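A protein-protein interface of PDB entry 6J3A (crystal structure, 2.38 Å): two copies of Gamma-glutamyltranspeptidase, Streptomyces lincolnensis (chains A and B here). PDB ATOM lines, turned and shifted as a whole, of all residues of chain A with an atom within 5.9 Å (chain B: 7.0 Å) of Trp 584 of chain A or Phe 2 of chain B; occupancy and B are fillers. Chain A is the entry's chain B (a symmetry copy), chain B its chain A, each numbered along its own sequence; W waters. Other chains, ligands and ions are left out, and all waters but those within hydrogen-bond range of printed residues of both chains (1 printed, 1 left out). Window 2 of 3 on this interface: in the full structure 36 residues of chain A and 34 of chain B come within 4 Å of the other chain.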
ATOM      1  N   THR A   4     -23.843 -16.474 -32.383  1.00  0.00           N
ATOM      2  CA  THR A   4     -24.610 -17.444 -31.605  1.00  0.00           C
ATOM      3  C   THR A   4     -25.740 -16.790 -30.821  1.00  0.00           C
ATOM      4  O   THR A   4     -26.727 -17.455 -30.487  1.00  0.00           O
ATOM      5  CB  THR A   4     -23.703 -18.216 -30.627  1.00  0.00           C
ATOM      6  OG1 THR A   4     -23.078 -17.301 -29.721  1.00  0.00           O
ATOM      7  CG2 THR A   4     -22.642 -19.035 -31.398  1.00  0.00           C
ATOM      8  N   ALA A 383     -15.805 -26.860 -20.668  1.00  0.00           N
ATOM      9  CA  ALA A 383     -16.989 -27.131 -21.482  1.00  0.00           C
ATOM     10  C   ALA A 383     -16.898 -28.505 -22.158  1.00  0.00           C
ATOM     11  O   ALA A 383     -16.488 -28.625 -23.317  1.00  0.00           O
ATOM     12  CB  ALA A 383     -17.162 -26.031 -22.516  1.00  0.00           C
ATOM     13  N   ILE A 533     -16.638 -12.166 -29.233  1.00  0.00           N
ATOM     14  CA  ILE A 533     -16.756 -13.306 -28.321  1.00  0.00           C
ATOM     15  C   ILE A 533     -16.781 -14.652 -29.063  1.00  0.00           C
ATOM     16  O   ILE A 533     -16.021 -15.564 -28.739  1.00  0.00           O
ATOM     17  CB  ILE A 533     -18.001 -13.158 -27.423  1.00  0.00           C
ATOM     18  CG1 ILE A 533     -17.801 -11.963 -26.468  1.00  0.00           C
ATOM     19  CG2 ILE A 533     -18.245 -14.434 -26.631  1.00  0.00           C
ATOM     20  CD1 ILE A 533     -18.955 -11.643 -25.536  1.00  0.00           C
ATOM     21  N   ASP A 534     -17.670 -14.766 -30.038  1.00  0.00           N
ATOM     22  CA  ASP A 534     -17.754 -15.957 -30.887  1.00  0.00           C
ATOM     23  C   ASP A 534     -16.408 -16.348 -31.490  1.00  0.00           C
ATOM     24  O   ASP A 534     -16.088 -17.525 -31.534  1.00  0.00           O
ATOM     25  CB  ASP A 534     -18.761 -15.761 -32.039  1.00  0.00           C
ATOM     26  CG  ASP A 534     -20.195 -16.130 -31.667  1.00  0.00           C
ATOM     27  OD1 ASP A 534     -20.554 -16.211 -30.468  1.00  0.00           O
ATOM     28  OD2 ASP A 534     -20.971 -16.338 -32.617  1.00  0.00           O
ATOM     29  N   GLU A 560      -8.594 -23.135 -30.483  1.00  0.00           N
ATOM     30  CA  GLU A 560      -9.866 -23.800 -30.763  1.00  0.00           C
ATOM     31  C   GLU A 560      -9.802 -24.499 -32.118  1.00  0.00           C
ATOM     32  O   GLU A 560      -9.067 -24.074 -33.020  1.00  0.00           O
ATOM     33  CB  GLU A 560     -11.012 -22.798 -30.716  1.00  0.00           C
ATOM     34  CG  GLU A 560     -11.221 -22.250 -29.317  1.00  0.00           C
ATOM     35  CD  GLU A 560     -12.502 -21.461 -29.155  1.00  0.00           C
ATOM     36  OE1 GLU A 560     -13.286 -21.771 -28.236  1.00  0.00           O
ATOM     37  OE2 GLU A 560     -12.732 -20.514 -29.926  1.00  0.00           O
ATOM     38  N   ALA A 561     -10.565 -25.582 -32.250  1.00  0.00           N
ATOM     39  CA  ALA A 561     -10.557 -26.397 -33.469  1.00  0.00           C
ATOM     40  C   ALA A 561     -11.121 -25.662 -34.682  1.00  0.00           C
ATOM     41  O   ALA A 561     -10.864 -26.066 -35.810  1.00  0.00           O
ATOM     42  CB  ALA A 561     -11.322 -27.693 -33.247  1.00  0.00           C
ATOM     43  N   ARG A 562     -11.876 -24.586 -34.445  1.00  0.00           N
ATOM     44  CA  ARG A 562     -12.528 -23.792 -35.523  1.00  0.00           C
ATOM     45  C   ARG A 562     -11.661 -22.636 -36.050  1.00  0.00           C
ATOM     46  O   ARG A 562     -12.039 -21.972 -37.007  1.00  0.00           O
ATOM     47  CB  ARG A 562     -13.958 -23.309 -35.146  1.00  0.00           C
ATOM     48  CG  ARG A 562     -14.297 -23.285 -33.662  1.00  0.00           C
ATOM     49  CD  ARG A 562     -15.765 -23.055 -33.370  1.00  0.00           C
ATOM     50  NE  ARG A 562     -16.127 -21.673 -33.590  1.00  0.00           N
ATOM     51  CZ  ARG A 562     -15.811 -20.645 -32.804  1.00  0.00           C
ATOM     52  NH1 ARG A 562     -15.101 -20.790 -31.691  1.00  0.00           N
ATOM     53  NH2 ARG A 562     -16.214 -19.439 -33.163  1.00  0.00           N
ATOM     54  N   PRO A 582     -11.027 -28.313 -28.143  1.00  0.00           N
ATOM     55  CA  PRO A 582     -12.338 -28.427 -28.786  1.00  0.00           C
ATOM     56  C   PRO A 582     -12.835 -27.112 -29.385  1.00  0.00           C
ATOM     57  O   PRO A 582     -12.395 -26.038 -28.950  1.00  0.00           O
ATOM     58  CB  PRO A 582     -13.270 -28.888 -27.646  1.00  0.00           C
ATOM     59  CG  PRO A 582     -12.373 -29.409 -26.593  1.00  0.00           C
ATOM     60  CD  PRO A 582     -11.112 -28.604 -26.699  1.00  0.00           C
ATOM     61  N   PRO A 583     -13.777 -27.199 -30.351  1.00  0.00           N
ATOM     62  CA  PRO A 583     -14.239 -26.029 -31.106  1.00  0.00           C
ATOM     63  C   PRO A 583     -14.706 -24.873 -30.228  1.00  0.00           C
ATOM     64  O   PRO A 583     -14.392 -23.722 -30.521  1.00  0.00           O
ATOM     65  CB  PRO A 583     -15.432 -26.564 -31.918  1.00  0.00           C
ATOM     66  CG  PRO A 583     -15.339 -28.045 -31.863  1.00  0.00           C
ATOM     67  CD  PRO A 583     -14.637 -28.376 -30.590  1.00  0.00           C
ATOM     68  N   TRP A 584     -15.446 -25.188 -29.167  1.00  0.00           N
ATOM     69  CA  TRP A 584     -16.059 -24.164 -28.322  1.00  0.00           C
ATOM     70  C   TRP A 584     -15.540 -24.309 -26.896  1.00  0.00           C
ATOM     71  O   TRP A 584     -16.273 -24.725 -26.002  1.00  0.00           O
ATOM     72  CB  TRP A 584     -17.589 -24.286 -28.381  1.00  0.00           C
ATOM     73  CG  TRP A 584     -18.150 -24.007 -29.741  1.00  0.00           C
ATOM     74  CD1 TRP A 584     -18.508 -24.930 -30.683  1.00  0.00           C
ATOM     75  CD2 TRP A 584     -18.410 -22.721 -30.319  1.00  0.00           C
ATOM     76  NE1 TRP A 584     -18.975 -24.298 -31.816  1.00  0.00           N
ATOM     77  CE2 TRP A 584     -18.928 -22.943 -31.616  1.00  0.00           C
ATOM     78  CE3 TRP A 584     -18.262 -21.404 -29.865  1.00  0.00           C
ATOM     79  CZ2 TRP A 584     -19.292 -21.897 -32.464  1.00  0.00           C
ATOM     80  CZ3 TRP A 584     -18.620 -20.366 -30.704  1.00  0.00           C
ATOM     81  CH2 TRP A 584     -19.130 -20.616 -31.994  1.00  0.00           C
ATOM     82  N   SER A 585     -14.273 -23.939 -26.704  1.00  0.00           N
ATOM     83  CA  SER A 585     -13.517 -24.232 -25.469  1.00  0.00           C
ATOM     84  C   SER A 585     -12.673 -23.102 -24.860  1.00  0.00           C
ATOM     85  O   SER A 585     -12.279 -23.205 -23.700  1.00  0.00           O
ATOM     86  CB  SER A 585     -12.575 -25.399 -25.734  1.00  0.00           C
ATOM     87  OG  SER A 585     -11.607 -25.045 -26.710  1.00  0.00           O
ATOM     88  N   GLU A 586     -12.411 -22.029 -25.602  1.00  0.00           N
ATOM     89  CA  GLU A 586     -11.516 -20.954 -25.146  1.00  0.00           C
ATOM     90  C   GLU A 586     -12.293 -19.664 -24.886  1.00  0.00           C
ATOM     91  O   GLU A 586     -12.843 -19.072 -25.807  1.00  0.00           O
ATOM     92  CB  GLU A 586     -10.435 -20.707 -26.193  1.00  0.00           C
ATOM     93  CG  GLU A 586      -9.538 -21.916 -26.461  1.00  0.00           C
ATOM     94  CD  GLU A 586      -8.512 -22.132 -25.371  1.00  0.00           C
ATOM     95  OE1 GLU A 586      -8.321 -23.288 -24.894  1.00  0.00           O
ATOM     96  OE2 GLU A 586      -7.900 -21.108 -24.999  1.00  0.00           O
ATOM     97  N   ARG A 588     -14.614 -17.446 -21.541  1.00  0.00           N
ATOM     98  CA  ARG A 588     -15.992 -17.289 -21.028  1.00  0.00           C
ATOM     99  C   ARG A 588     -16.314 -15.795 -20.903  1.00  0.00           C
ATOM    100  O   ARG A 588     -16.744 -15.316 -19.849  1.00  0.00           O
ATOM    101  CB  ARG A 588     -16.255 -18.008 -19.678  1.00  0.00           C
ATOM    102  CG  ARG A 588     -15.480 -19.277 -19.349  1.00  0.00           C
ATOM    103  CD  ARG A 588     -16.085 -20.561 -19.888  1.00  0.00           C
ATOM    104  NE  ARG A 588     -15.347 -20.972 -21.077  1.00  0.00           N
ATOM    105  CZ  ARG A 588     -15.054 -22.219 -21.444  1.00  0.00           C
ATOM    106  NH1 ARG A 588     -14.361 -22.394 -22.556  1.00  0.00           N
ATOM    107  NH2 ARG A 588     -15.427 -23.283 -20.736  1.00  0.00           N
ATOM    108  N   PRO A 607     -20.941 -18.236 -25.626  1.00  0.00           N
ATOM    109  CA  PRO A 607     -21.821 -19.387 -25.766  1.00  0.00           C
ATOM    110  C   PRO A 607     -21.250 -20.734 -25.282  1.00  0.00           C
ATOM    111  O   PRO A 607     -22.002 -21.707 -25.169  1.00  0.00           O
ATOM    112  CB  PRO A 607     -22.066 -19.431 -27.268  1.00  0.00           C
ATOM    113  CG  PRO A 607     -20.778 -18.968 -27.850  1.00  0.00           C
ATOM    114  CD  PRO A 607     -20.172 -18.002 -26.864  1.00  0.00           C
ATOM    115  N   ARG A 608     -19.954 -20.784 -24.991  1.00  0.00           N
ATOM    116  CA  ARG A 608     -19.274 -22.043 -24.733  1.00  0.00           C
ATOM    117  C   ARG A 608     -19.587 -22.482 -23.313  1.00  0.00           C
ATOM    118  O   ARG A 608     -19.399 -21.702 -22.379  1.00  0.00           O
ATOM    119  CB  ARG A 608     -17.761 -21.909 -24.888  1.00  0.00           C
ATOM    120  CG  ARG A 608     -17.268 -21.223 -26.146  1.00  0.00           C
ATOM    121  CD  ARG A 608     -15.829 -20.794 -25.934  1.00  0.00           C
ATOM    122  NE  ARG A 608     -15.231 -20.254 -27.145  1.00  0.00           N
ATOM    123  CZ  ARG A 608     -15.428 -19.021 -27.609  1.00  0.00           C
ATOM    124  NH1 ARG A 608     -16.227 -18.161 -26.966  1.00  0.00           N
ATOM    125  NH2 ARG A 608     -14.820 -18.638 -28.727  1.00  0.00           N
ATOM    126  N   GLY A 609     -20.031 -23.731 -23.169  1.00  0.00           N
ATOM    127  CA  GLY A 609     -20.476 -24.275 -21.890  1.00  0.00           C
ATOM    128  C   GLY A 609     -21.935 -23.964 -21.591  1.00  0.00           C
ATOM    129  O   GLY A 609     -22.385 -24.190 -20.478  1.00  0.00           O
ATOM    130  N   MET A 610     -22.670 -23.481 -22.597  1.00  0.00           N
ATOM    131  CA  MET A 610     -24.084 -23.083 -22.492  1.00  0.00           C
ATOM    132  C   MET A 610     -24.497 -22.629 -21.092  1.00  0.00           C
ATOM    133  O   MET A 610     -25.299 -23.278 -20.409  1.00  0.00           O
ATOM    134  CB  MET A 610     -25.024 -24.187 -23.003  1.00  0.00           C
ATOM    135  CG  MET A 610     -24.352 -25.404 -23.572  1.00  0.00           C
ATOM    136  SD  MET A 610     -23.414 -25.150 -25.080  1.00  0.00           S
ATOM    137  CE  MET A 610     -22.344 -26.588 -24.910  1.00  0.00           C
ATOM    138  N   MET B   1     -23.469 -31.718 -26.186  1.00  0.00           N
ATOM    139  CA  MET B   1     -23.274 -31.208 -27.583  1.00  0.00           C
ATOM    140  C   MET B   1     -23.586 -29.701 -27.667  1.00  0.00           C
ATOM    141  O   MET B   1     -24.585 -29.244 -27.108  1.00  0.00           O
ATOM    142  CB  MET B   1     -24.146 -31.996 -28.567  1.00  0.00           C
ATOM    143  N   PHE B   2     -22.728 -28.942 -28.362  1.00  0.00           N
ATOM    144  CA  PHE B   2     -22.817 -27.461 -28.407  1.00  0.00           C
ATOM    145  C   PHE B   2     -24.130 -26.915 -28.982  1.00  0.00           C
ATOM    146  O   PHE B   2     -24.563 -27.317 -30.062  1.00  0.00           O
ATOM    147  CB  PHE B   2     -21.648 -26.839 -29.184  1.00  0.00           C
ATOM    148  CG  PHE B   2     -21.687 -25.318 -29.247  1.00  0.00           C
ATOM    149  CD1 PHE B   2     -21.356 -24.545 -28.127  1.00  0.00           C
ATOM    150  CD2 PHE B   2     -22.054 -24.659 -30.414  1.00  0.00           C
ATOM    151  CE1 PHE B   2     -21.387 -23.151 -28.174  1.00  0.00           C
ATOM    152  CE2 PHE B   2     -22.081 -23.269 -30.463  1.00  0.00           C
ATOM    153  CZ  PHE B   2     -21.743 -22.514 -29.345  1.00  0.00           C
ATOM    154  N   THR B   3     -24.736 -25.993 -28.231  1.00  0.00           N
ATOM    155  CA  THR B   3     -25.890 -25.221 -28.672  1.00  0.00           C
ATOM    156  C   THR B   3     -25.566 -23.742 -28.555  1.00  0.00           C
ATOM    157  O   THR B   3     -24.830 -23.310 -27.660  1.00  0.00           O
ATOM    158  CB  THR B   3     -27.153 -25.518 -27.845  1.00  0.00           C
ATOM    159  OG1 THR B   3     -26.887 -25.291 -26.459  1.00  0.00           O
ATOM    160  CG2 THR B   3     -27.602 -26.953 -28.038  1.00  0.00           C
ATOM    161  N   THR B   4     -26.174 -22.974 -29.447  1.00  0.00           N
ATOM    162  CA  THR B   4     -25.888 -21.554 -29.613  1.00  0.00           C
ATOM    163  C   THR B   4     -26.278 -20.727 -28.384  1.00  0.00           C
ATOM    164  O   THR B   4     -25.746 -19.643 -28.165  1.00  0.00           O
ATOM    165  CB  THR B   4     -26.633 -20.994 -30.837  1.00  0.00           C
ATOM    166  OG1 THR B   4     -28.051 -21.145 -30.660  1.00  0.00           O
ATOM    167  CG2 THR B   4     -26.180 -21.706 -32.120  1.00  0.00           C
ATOM    168  N   ARG B   5     -27.227 -21.251 -27.613  1.00  0.00           N
ATOM    169  CA  ARG B   5     -27.608 -20.721 -26.311  1.00  0.00           C
ATOM    170  C   ARG B   5     -27.835 -21.903 -25.391  1.00  0.00           C
ATOM    171  O   ARG B   5     -27.825 -23.059 -25.824  1.00  0.00           O
ATOM    172  CB  ARG B   5     -28.891 -19.905 -26.398  1.00  0.00           C
ATOM    173  CG  ARG B   5     -28.754 -18.610 -27.171  1.00  0.00           C
ATOM    174  CD  ARG B   5     -29.705 -18.633 -28.340  1.00  0.00           C
ATOM    175  NE  ARG B   5     -29.374 -17.645 -29.354  1.00  0.00           N
ATOM    176  CZ  ARG B   5     -30.176 -16.673 -29.775  1.00  0.00           C
ATOM    177  NH1 ARG B   5     -29.754 -15.858 -30.717  1.00  0.00           N
ATOM    178  NH2 ARG B   5     -31.394 -16.502 -29.276  1.00  0.00           N
ATOM    179  N   ARG B 520     -35.245 -36.357 -29.294  1.00  0.00           N
ATOM    180  CA  ARG B 520     -33.874 -36.078 -28.851  1.00  0.00           C
ATOM    181  C   ARG B 520     -33.682 -36.404 -27.374  1.00  0.00           C
ATOM    182  O   ARG B 520     -34.596 -36.249 -26.562  1.00  0.00           O
ATOM    183  CB  ARG B 520     -33.491 -34.615 -29.118  1.00  0.00           C
ATOM    184  CG  ARG B 520     -33.293 -34.278 -30.590  1.00  0.00           C
ATOM    185  CD  ARG B 520     -33.110 -32.782 -30.784  1.00  0.00           C
ATOM    186  NE  ARG B 520     -31.762 -32.359 -30.402  1.00  0.00           N
ATOM    187  CZ  ARG B 520     -30.707 -32.296 -31.220  1.00  0.00           C
ATOM    188  NH1 ARG B 520     -30.803 -32.614 -32.518  1.00  0.00           N
ATOM    189  NH2 ARG B 520     -29.532 -31.899 -30.733  1.00  0.00           N
ATOM    190  N   GLY B 531     -31.346 -27.481 -28.561  1.00  0.00           N
ATOM    191  CA  GLY B 531     -30.740 -28.416 -29.505  1.00  0.00           C
ATOM    192  C   GLY B 531     -31.697 -28.743 -30.639  1.00  0.00           C
ATOM    193  O   GLY B 531     -31.271 -28.950 -31.785  1.00  0.00           O
ATOM    194  N   ASP B 534     -31.741 -25.319 -32.734  1.00  0.00           N
ATOM    195  CA  ASP B 534     -30.467 -25.309 -33.478  1.00  0.00           C
ATOM    196  C   ASP B 534     -30.464 -26.314 -34.616  1.00  0.00           C
ATOM    197  O   ASP B 534     -29.909 -26.032 -35.671  1.00  0.00           O
ATOM    198  CB  ASP B 534     -29.268 -25.632 -32.572  1.00  0.00           C
ATOM    199  CG  ASP B 534     -28.773 -24.432 -31.761  1.00  0.00           C
ATOM    200  OD1 ASP B 534     -29.501 -23.426 -31.592  1.00  0.00           O
ATOM    201  OD2 ASP B 534     -27.629 -24.524 -31.265  1.00  0.00           O
ATOM    202  N   TRP B 584     -27.954 -20.928 -41.656  1.00  0.00           N
ATOM    203  CA  TRP B 584     -28.781 -20.462 -40.543  1.00  0.00           C
ATOM    204  C   TRP B 584     -29.951 -19.638 -41.060  1.00  0.00           C
ATOM    205  O   TRP B 584     -29.983 -18.420 -40.881  1.00  0.00           O
ATOM    206  CB  TRP B 584     -27.915 -19.640 -39.579  1.00  0.00           C
ATOM    207  CG  TRP B 584     -26.847 -20.450 -38.914  1.00  0.00           C
ATOM    208  CD1 TRP B 584     -25.542 -20.538 -39.285  1.00  0.00           C
ATOM    209  CD2 TRP B 584     -27.000 -21.301 -37.767  1.00  0.00           C
ATOM    210  NE1 TRP B 584     -24.861 -21.384 -38.435  1.00  0.00           N
ATOM    211  CE2 TRP B 584     -25.732 -21.866 -37.495  1.00  0.00           C
ATOM    212  CE3 TRP B 584     -28.083 -21.639 -36.946  1.00  0.00           C
ATOM    213  CZ2 TRP B 584     -25.513 -22.747 -36.436  1.00  0.00           C
ATOM    214  CZ3 TRP B 584     -27.872 -22.516 -35.893  1.00  0.00           C
ATOM    215  CH2 TRP B 584     -26.592 -23.059 -35.642  1.00  0.00           C
HETATM  216  O   HOH W   1     -28.057 -15.307 -32.745  1.00  0.00           O
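The backbone NH (N) of Thr 3 of chain B is in hydrogen-bond range of the side-chain sulfur (SD) of Met 610 of chain A.
The guanidinium group (NE) of Arg 5 of chain B sits at hydrogen-bond distance from the backbone carbonyl oxygen (O) of Thr 4 of chain A (2.9 Å).
O of Thr 4 of chain A lies close to O of Thr 4 of chain B.
The backbone carbonyl oxygen (O) of Arg 5 of chain B lies within hydrogen-bond range of the side-chain hydroxyl (OG1) of Thr 3 of chain B, 2.5 Å away.
The backbone NH of Thr 4 of chain B lies within hydrogen-bond range of the side-chain carboxylate of Asp 534 of chain B, 2.8 Å away.
OD1 of Asp 534 of chain A sits at hydrogen-bond distance from OG1 of Thr 4 of chain A (2.8 Å).
Among the printed residues, pairs that only touch across the chains: Trp 584 of chain A with Phe 2 of chain B, Pro 607 of chain A with Phe 2 of chain B, Met 610 of chain A with Phe 2 of chain B and Pro 607 of chain A with Thr 4 of chain B.
Printed residues of chain B within 4 Å of Met 610 of chain A: Phe 2 (3.6 Å) and Thr 3 (3.5 Å).
Of the printed residues of chain A, Arg 5 of chain B touches Thr 4.
The nearest residue of chain B that does not touch Trp 584 of chain A is Thr 3 of chain B (6.8 Å).
The nearest residue of chain A that does not touch Phe 2 of chain B is Thr 4 of chain A (4.1 Å).
Of the 9 printed residues of chain B, 4 touch a printed residue of chain A.
Hydrophobic or aromatic side chains of chain B that line the printed part of chain A: Phe 2.
Hydrophobic or aromatic side chains of chain A that line the printed part of chain B: Trp 584, Pro 607 and Met 610.
Thr 4 of chain A touches its own counterpart, Thr 4 of chain B.
Water W1 bridges the guanidinium group (NH1) of Arg 5 of chain B (2.7 Å) and the backbone carbonyl oxygen (O) of Thr 4 of chain A (3.4 Å).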
